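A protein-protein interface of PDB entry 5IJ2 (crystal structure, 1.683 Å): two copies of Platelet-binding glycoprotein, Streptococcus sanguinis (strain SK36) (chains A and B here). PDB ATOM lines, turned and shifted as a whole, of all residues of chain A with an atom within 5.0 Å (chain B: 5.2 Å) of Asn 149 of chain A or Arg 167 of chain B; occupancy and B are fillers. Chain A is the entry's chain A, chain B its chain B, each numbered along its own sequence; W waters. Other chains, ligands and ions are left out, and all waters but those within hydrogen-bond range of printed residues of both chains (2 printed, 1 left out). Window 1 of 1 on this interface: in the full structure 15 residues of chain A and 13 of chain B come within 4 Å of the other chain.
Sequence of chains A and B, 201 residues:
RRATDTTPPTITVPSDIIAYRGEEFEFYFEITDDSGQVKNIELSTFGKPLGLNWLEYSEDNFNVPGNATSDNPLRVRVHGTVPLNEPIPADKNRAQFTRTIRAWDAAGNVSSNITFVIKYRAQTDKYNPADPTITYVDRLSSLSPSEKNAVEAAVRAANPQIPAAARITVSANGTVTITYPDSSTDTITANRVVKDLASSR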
ATOM      1  N   PRO A 145     -10.826  26.842  -1.593  1.00  0.00           N
ATOM      2  CA  PRO A 145      -9.779  27.218  -2.558  1.00  0.00           C
ATOM      3  C   PRO A 145     -10.335  27.834  -3.829  1.00  0.00           C
ATOM      4  O   PRO A 145      -9.775  28.818  -4.336  1.00  0.00           O
ATOM      5  CB  PRO A 145      -9.047  25.894  -2.816  1.00  0.00           C
ATOM      6  CG  PRO A 145      -9.275  25.109  -1.552  1.00  0.00           C
ATOM      7  CD  PRO A 145     -10.653  25.473  -1.084  1.00  0.00           C
ATOM      8  N   SER A 146     -11.453  27.320  -4.346  1.00  0.00           N
ATOM      9  CA  SER A 146     -12.024  27.917  -5.548  1.00  0.00           C
ATOM     10  C   SER A 146     -12.567  29.307  -5.277  1.00  0.00           C
ATOM     11  O   SER A 146     -12.549  30.155  -6.174  1.00  0.00           O
ATOM     12  CB  SER A 146     -13.143  27.055  -6.118  1.00  0.00           C
ATOM     13  OG  SER A 146     -14.202  26.948  -5.190  1.00  0.00           O
ATOM     14  N   GLU A 147     -13.062  29.557  -4.063  1.00  0.00           N
ATOM     15  CA  GLU A 147     -13.518  30.912  -3.751  1.00  0.00           C
ATOM     16  C   GLU A 147     -12.344  31.873  -3.655  1.00  0.00           C
ATOM     17  O   GLU A 147     -12.454  33.022  -4.089  1.00  0.00           O
ATOM     18  CB  GLU A 147     -14.323  30.927  -2.460  1.00  0.00           C
ATOM     19  CG  GLU A 147     -15.664  30.259  -2.619  1.00  0.00           C
ATOM     20  CD  GLU A 147     -16.258  29.812  -1.315  1.00  0.00           C
ATOM     21  OE1 GLU A 147     -15.557  29.862  -0.276  1.00  0.00           O
ATOM     22  OE2 GLU A 147     -17.442  29.405  -1.342  1.00  0.00           O
ATOM     23  N   LYS A 148     -11.217  31.434  -3.093  1.00  0.00           N
ATOM     24  CA  LYS A 148     -10.053  32.319  -3.065  1.00  0.00           C
ATOM     25  C   LYS A 148      -9.540  32.593  -4.472  1.00  0.00           C
ATOM     26  O   LYS A 148      -9.225  33.735  -4.807  1.00  0.00           O
ATOM     27  CB  LYS A 148      -8.953  31.726  -2.189  1.00  0.00           C
ATOM     28  CG  LYS A 148      -9.339  31.630  -0.759  1.00  0.00           C
ATOM     29  CD  LYS A 148      -8.204  31.110   0.103  1.00  0.00           C
ATOM     30  CE  LYS A 148      -8.731  30.854   1.518  1.00  0.00           C
ATOM     31  NZ  LYS A 148      -7.787  30.049   2.372  1.00  0.00           N
ATOM     32  N   ASN A 149      -9.479  31.565  -5.322  1.00  0.00           N
ATOM     33  CA  ASN A 149      -9.137  31.775  -6.731  1.00  0.00           C
ATOM     34  C   ASN A 149     -10.056  32.806  -7.368  1.00  0.00           C
ATOM     35  O   ASN A 149      -9.609  33.705  -8.095  1.00  0.00           O
ATOM     36  CB  ASN A 149      -9.267  30.466  -7.534  1.00  0.00           C
ATOM     37  CG  ASN A 149      -8.116  29.520  -7.331  1.00  0.00           C
ATOM     38  OD1 ASN A 149      -7.115  29.854  -6.706  1.00  0.00           O
ATOM     39  ND2 ASN A 149      -8.249  28.306  -7.896  1.00  0.00           N
ATOM     40  N   ALA A 150     -11.363  32.644  -7.135  1.00  0.00           N
ATOM     41  CA  ALA A 150     -12.357  33.533  -7.721  1.00  0.00           C
ATOM     42  C   ALA A 150     -12.152  34.965  -7.257  1.00  0.00           C
ATOM     43  O   ALA A 150     -12.170  35.897  -8.073  1.00  0.00           O
ATOM     44  CB  ALA A 150     -13.771  33.063  -7.356  1.00  0.00           C
ATOM     45  N   VAL A 151     -11.964  35.159  -5.946  1.00  0.00           N
ATOM     46  CA  VAL A 151     -11.693  36.510  -5.424  1.00  0.00           C
ATOM     47  C   VAL A 151     -10.484  37.108  -6.122  1.00  0.00           C
ATOM     48  O   VAL A 151     -10.531  38.221  -6.677  1.00  0.00           O
ATOM     49  CB  VAL A 151     -11.464  36.460  -3.904  1.00  0.00           C
ATOM     50  CG1 VAL A 151     -10.817  37.783  -3.432  1.00  0.00           C
ATOM     51  CG2 VAL A 151     -12.759  36.165  -3.134  1.00  0.00           C
ATOM     52  N   GLU A 152      -9.367  36.384  -6.091  1.00  0.00           N
ATOM     53  CA  GLU A 152      -8.167  36.870  -6.758  1.00  0.00           C
ATOM     54  C   GLU A 152      -8.451  37.280  -8.201  1.00  0.00           C
ATOM     55  O   GLU A 152      -8.052  38.362  -8.639  1.00  0.00           O
ATOM     56  CB  GLU A 152      -7.076  35.810  -6.705  1.00  0.00           C
ATOM     57  CG  GLU A 152      -5.788  36.303  -7.338  1.00  0.00           C
ATOM     58  CD  GLU A 152      -4.661  35.281  -7.302  1.00  0.00           C
ATOM     59  OE1 GLU A 152      -4.764  34.266  -6.578  1.00  0.00           O
ATOM     60  OE2 GLU A 152      -3.646  35.494  -7.999  1.00  0.00           O
ATOM     61  N   ALA A 153      -9.133  36.418  -8.964  1.00  0.00           N
ATOM     62  CA  ALA A 153      -9.430  36.736 -10.362  1.00  0.00           C
ATOM     63  C   ALA A 153     -10.288  37.991 -10.479  1.00  0.00           C
ATOM     64  O   ALA A 153     -10.091  38.803 -11.395  1.00  0.00           O
ATOM     65  CB  ALA A 153     -10.125  35.541 -11.023  1.00  0.00           C
ATOM     66  N   ALA A 154     -11.242  38.169  -9.560  1.00  0.00           N
ATOM     67  CA  ALA A 154     -12.100  39.353  -9.582  1.00  0.00           C
ATOM     68  C   ALA A 154     -11.304  40.612  -9.266  1.00  0.00           C
ATOM     69  O   ALA A 154     -11.465  41.644  -9.930  1.00  0.00           O
ATOM     70  CB  ALA A 154     -13.239  39.203  -8.583  1.00  0.00           C
ATOM     71  N   ILE A 168      -1.565  39.096  -5.626  1.00  0.00           N
ATOM     72  CA  ILE A 168      -2.829  39.238  -4.915  1.00  0.00           C
ATOM     73  C   ILE A 168      -3.037  37.995  -4.065  1.00  0.00           C
ATOM     74  O   ILE A 168      -3.097  36.881  -4.598  1.00  0.00           O
ATOM     75  CB  ILE A 168      -3.989  39.428  -5.902  1.00  0.00           C
ATOM     76  CG1 ILE A 168      -3.793  40.665  -6.771  1.00  0.00           C
ATOM     77  CG2 ILE A 168      -5.309  39.514  -5.181  1.00  0.00           C
ATOM     78  CD1 ILE A 168      -4.752  40.670  -7.930  1.00  0.00           C
ATOM     79  N   THR A 169      -3.159  38.170  -2.751  1.00  0.00           N
ATOM     80  CA  THR A 169      -3.413  37.054  -1.859  1.00  0.00           C
ATOM     81  C   THR A 169      -4.757  37.280  -1.192  1.00  0.00           C
ATOM     82  O   THR A 169      -5.277  38.406  -1.143  1.00  0.00           O
ATOM     83  CB  THR A 169      -2.304  36.890  -0.807  1.00  0.00           C
ATOM     84  OG1 THR A 169      -1.983  38.169  -0.226  1.00  0.00           O
ATOM     85  CG2 THR A 169      -1.035  36.323  -1.440  1.00  0.00           C
ATOM     86  N   VAL A 170      -5.340  36.182  -0.716  1.00  0.00           N
ATOM     87  CA  VAL A 170      -6.677  36.182  -0.140  1.00  0.00           C
ATOM     88  C   VAL A 170      -6.648  35.372   1.148  1.00  0.00           C
ATOM     89  O   VAL A 170      -6.206  34.211   1.165  1.00  0.00           O
ATOM     90  CB  VAL A 170      -7.711  35.592  -1.122  1.00  0.00           C
ATOM     91  CG1 VAL A 170      -9.125  35.770  -0.575  1.00  0.00           C
ATOM     92  CG2 VAL A 170      -7.590  36.252  -2.485  1.00  0.00           C
ATOM     93  N   ARG B 156       1.248  25.935 -12.176  1.00  0.00           N
ATOM     94  CA  ARG B 156      -0.015  25.787 -12.895  1.00  0.00           C
ATOM     95  C   ARG B 156       0.207  25.301 -14.332  1.00  0.00           C
ATOM     96  O   ARG B 156      -0.467  24.365 -14.789  1.00  0.00           O
ATOM     97  CB  ARG B 156      -0.792  27.101 -12.859  1.00  0.00           C
ATOM     98  CG  ARG B 156      -2.179  27.030 -13.529  1.00  0.00           C
ATOM     99  CD  ARG B 156      -3.116  26.113 -12.715  1.00  0.00           C
ATOM    100  NE  ARG B 156      -3.500  26.722 -11.439  1.00  0.00           N
ATOM    101  CZ  ARG B 156      -4.378  26.182 -10.598  1.00  0.00           C
ATOM    102  NH1 ARG B 156      -4.947  25.018 -10.894  1.00  0.00           N
ATOM    103  NH2 ARG B 156      -4.671  26.796  -9.457  1.00  0.00           N
ATOM    104  N   ALA B 164      -8.675  23.161 -11.777  1.00  0.00           N
ATOM    105  CA  ALA B 164      -8.516  24.611 -11.845  1.00  0.00           C
ATOM    106  C   ALA B 164      -8.869  25.248 -10.509  1.00  0.00           C
ATOM    107  O   ALA B 164      -8.261  26.251 -10.113  1.00  0.00           O
ATOM    108  CB  ALA B 164      -9.384  25.177 -12.968  1.00  0.00           C
ATOM    109  N   ALA B 165      -9.790  24.630  -9.777  1.00  0.00           N
ATOM    110  CA  ALA B 165     -10.262  25.087  -8.481  1.00  0.00           C
ATOM    111  C   ALA B 165      -9.254  24.883  -7.354  1.00  0.00           C
ATOM    112  O   ALA B 165      -9.447  25.450  -6.272  1.00  0.00           O
ATOM    113  CB  ALA B 165     -11.574  24.368  -8.144  1.00  0.00           C
ATOM    114  N   ALA B 166      -8.205  24.087  -7.544  1.00  0.00           N
ATOM    115  CA  ALA B 166      -7.191  24.007  -6.511  1.00  0.00           C
ATOM    116  C   ALA B 166      -6.486  25.346  -6.429  1.00  0.00           C
ATOM    117  O   ALA B 166      -6.383  26.063  -7.428  1.00  0.00           O
ATOM    118  CB  ALA B 166      -6.186  22.904  -6.829  1.00  0.00           C
ATOM    119  N   ARG B 167      -6.013  25.689  -5.241  1.00  0.00           N
ATOM    120  CA  ARG B 167      -5.299  26.944  -5.051  1.00  0.00           C
ATOM    121  C   ARG B 167      -3.836  26.659  -4.766  1.00  0.00           C
ATOM    122  O   ARG B 167      -3.508  25.864  -3.881  1.00  0.00           O
ATOM    123  CB  ARG B 167      -5.885  27.767  -3.915  1.00  0.00           C
ATOM    124  CG  ARG B 167      -5.233  29.136  -3.861  1.00  0.00           C
ATOM    125  CD  ARG B 167      -6.218  30.101  -3.346  1.00  0.00           C
ATOM    126  NE  ARG B 167      -5.618  31.403  -3.113  1.00  0.00           N
ATOM    127  CZ  ARG B 167      -5.564  32.378  -4.011  1.00  0.00           C
ATOM    128  NH1 ARG B 167      -6.090  32.196  -5.226  1.00  0.00           N
ATOM    129  NH2 ARG B 167      -4.989  33.549  -3.681  1.00  0.00           N
ATOM    130  N   ILE B 168      -2.964  27.326  -5.512  1.00  0.00           N
ATOM    131  CA  ILE B 168      -1.523  27.167  -5.386  1.00  0.00           C
ATOM    132  C   ILE B 168      -0.983  28.380  -4.629  1.00  0.00           C
ATOM    133  O   ILE B 168      -1.138  29.509  -5.098  1.00  0.00           O
ATOM    134  CB  ILE B 168      -0.880  27.066  -6.779  1.00  0.00           C
ATOM    135  CG1 ILE B 168      -1.485  25.893  -7.581  1.00  0.00           C
ATOM    136  CG2 ILE B 168       0.647  26.958  -6.669  1.00  0.00           C
ATOM    137  CD1 ILE B 168      -1.193  25.970  -9.122  1.00  0.00           C
ATOM    138  N   THR B 169      -0.363  28.160  -3.469  1.00  0.00           N
ATOM    139  CA  THR B 169       0.277  29.237  -2.722  1.00  0.00           C
ATOM    140  C   THR B 169       1.780  29.000  -2.676  1.00  0.00           C
ATOM    141  O   THR B 169       2.266  27.878  -2.871  1.00  0.00           O
ATOM    142  CB  THR B 169      -0.279  29.340  -1.301  1.00  0.00           C
ATOM    143  OG1 THR B 169      -0.264  28.040  -0.693  1.00  0.00           O
ATOM    144  CG2 THR B 169      -1.718  29.826  -1.333  1.00  0.00           C
ATOM    145  N   THR B 177       2.458  25.117  -1.802  1.00  0.00           N
ATOM    146  CA  THR B 177       1.341  24.335  -1.296  1.00  0.00           C
ATOM    147  C   THR B 177       0.238  24.344  -2.338  1.00  0.00           C
ATOM    148  O   THR B 177      -0.120  25.408  -2.860  1.00  0.00           O
ATOM    149  CB  THR B 177       0.831  24.908   0.025  1.00  0.00           C
ATOM    150  OG1 THR B 177       1.911  24.888   0.964  1.00  0.00           O
ATOM    151  CG2 THR B 177      -0.332  24.077   0.576  1.00  0.00           C
ATOM    152  N   ILE B 178      -0.286  23.160  -2.660  1.00  0.00           N
ATOM    153  CA  ILE B 178      -1.460  23.036  -3.500  1.00  0.00           C
ATOM    154  C   ILE B 178      -2.572  22.565  -2.595  1.00  0.00           C
ATOM    155  O   ILE B 178      -2.448  21.515  -1.951  1.00  0.00           O
ATOM    156  CB  ILE B 178      -1.226  22.043  -4.649  1.00  0.00           C
ATOM    157  CG1 ILE B 178      -0.020  22.520  -5.465  1.00  0.00           C
ATOM    158  CG2 ILE B 178      -2.501  21.904  -5.486  1.00  0.00           C
ATOM    159  CD1 ILE B 178       0.306  21.653  -6.666  1.00  0.00           C
ATOM    160  N   THR B 179      -3.654  23.340  -2.521  1.00  0.00           N
ATOM    161  CA  THR B 179      -4.793  22.974  -1.693  1.00  0.00           C
ATOM    162  C   THR B 179      -5.928  22.595  -2.634  1.00  0.00           C
ATOM    163  O   THR B 179      -6.426  23.430  -3.387  1.00  0.00           O
ATOM    164  CB  THR B 179      -5.176  24.104  -0.739  1.00  0.00           C
ATOM    165  OG1 THR B 179      -4.023  24.452   0.026  1.00  0.00           O
ATOM    166  CG2 THR B 179      -6.291  23.623   0.234  1.00  0.00           C
ATOM    167  N   TYR B 180      -6.283  21.318  -2.633  1.00  0.00           N
ATOM    168  CA  TYR B 180      -7.326  20.820  -3.508  1.00  0.00           C
ATOM    169  C   TYR B 180      -8.692  21.256  -3.009  1.00  0.00           C
ATOM    170  O   TYR B 180      -8.839  21.659  -1.857  1.00  0.00           O
ATOM    171  CB  TYR B 180      -7.221  19.293  -3.588  1.00  0.00           C
ATOM    172  CG  TYR B 180      -5.898  18.919  -4.200  1.00  0.00           C
ATOM    173  CD1 TYR B 180      -5.655  19.178  -5.538  1.00  0.00           C
ATOM    174  CD2 TYR B 180      -4.886  18.324  -3.443  1.00  0.00           C
ATOM    175  CE1 TYR B 180      -4.431  18.879  -6.111  1.00  0.00           C
ATOM    176  CE2 TYR B 180      -3.659  18.031  -4.006  1.00  0.00           C
ATOM    177  CZ  TYR B 180      -3.445  18.308  -5.335  1.00  0.00           C
ATOM    178  OH  TYR B 180      -2.226  18.017  -5.886  1.00  0.00           O
HETATM  179  O   HOH W   1      -4.096  29.129  -7.541  1.00  0.00           O
HETATM  180  O   HOH W   2     -10.843  28.396  -9.662  1.00  0.00           O
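The side-chain amide nitrogen (ND2) of Asn 149 of chain A lies within hydrogen-bond range of the backbone carbonyl oxygen (O) of Ala 165 of chain B (3.5 Å). The backbone carbonyl oxygen of Ala 164 of chain B is in hydrogen-bond range of the side-chain amide nitrogen of Asn 149 of chain A (3.0 Å). The side-chain carboxylate of Glu 152 of chain A lies close to the guanidinium group of Arg 167 of chain B. N of Ser 146 of chain A lies within hydrogen-bond range of O of Ala 165 of chain B (3.4 Å). ND2 of Asn 149 of chain A is in hydrogen-bond range of O of Ala 166 of chain B (3.0 Å). OD1 of Asn 149 of chain A is in hydrogen-bond range of NH1 of Arg 167 of chain B (3.0 Å).
O of Arg 167 of chain B sits at hydrogen-bond distance from N of Thr 179 of chain B (2.9 Å). The backbone carbonyl oxygen of Ala 166 of chain B is in hydrogen-bond range of the guanidinium group of Arg 156 of chain B, at 2.8 Å.
Ala 165 of chain B touches Pro 145 of chain A. Pro 145 of chain A touches Arg 167 of chain B (CB to CB, 3.8 Å). Pro 145 of chain A touches Thr 179 of chain B (CB to O, 3.6 Å). Pro 145 of chain A touches Tyr 180 of chain B (CG to O, 3.5 Å). CB of Lys 148 of chain A touches CD of Arg 167 of chain B, 3.4 Å away. Arg 167 of chain B touches Ile 168 of chain A. Arg 167 of chain B touches Val 170 of chain A (NH2 to CG2, 3.9 Å).
Of the printed residues of chain A, Ala 164 of chain B touches Asn 149 (3.0 Å). Arg 167 of chain B touches just these residues of chain A: Pro 145, Lys 148, Asn 149, Glu 152, Ile 168 and Val 170. Printed residues of chain A within 4 Å of Thr 179 of chain B: Pro 145.
Along chain B the printed residues that touch a printed residue of chain A span positions 164 to 180. Printed residues of chain A that touch a printed residue of chain B: Pro 145, Ser 146, Lys 148, Asn 149, Glu 152, Ile 168 and Val 170. Among the printed residues, Asp or Glu carboxylates within 4 Å of a Lys or Arg side-chain nitrogen of the other chain: Glu 152 of chain A with Arg 167 of chain B.
Positions printed for both chains: 168 and 169.
Water W1 lies within hydrogen-bond range of the backbone NH (N) of Ile 168 of chain B, the guanidinium group (NH2) of Arg 156 of chain B and the side-chain amide oxygen (OD1) of Asn 149 of chain A. Water W2 bridges the side-chain amide nitrogen of Asn 149 of chain A and the backbone carbonyl oxygen of Ala 164 of chain B.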
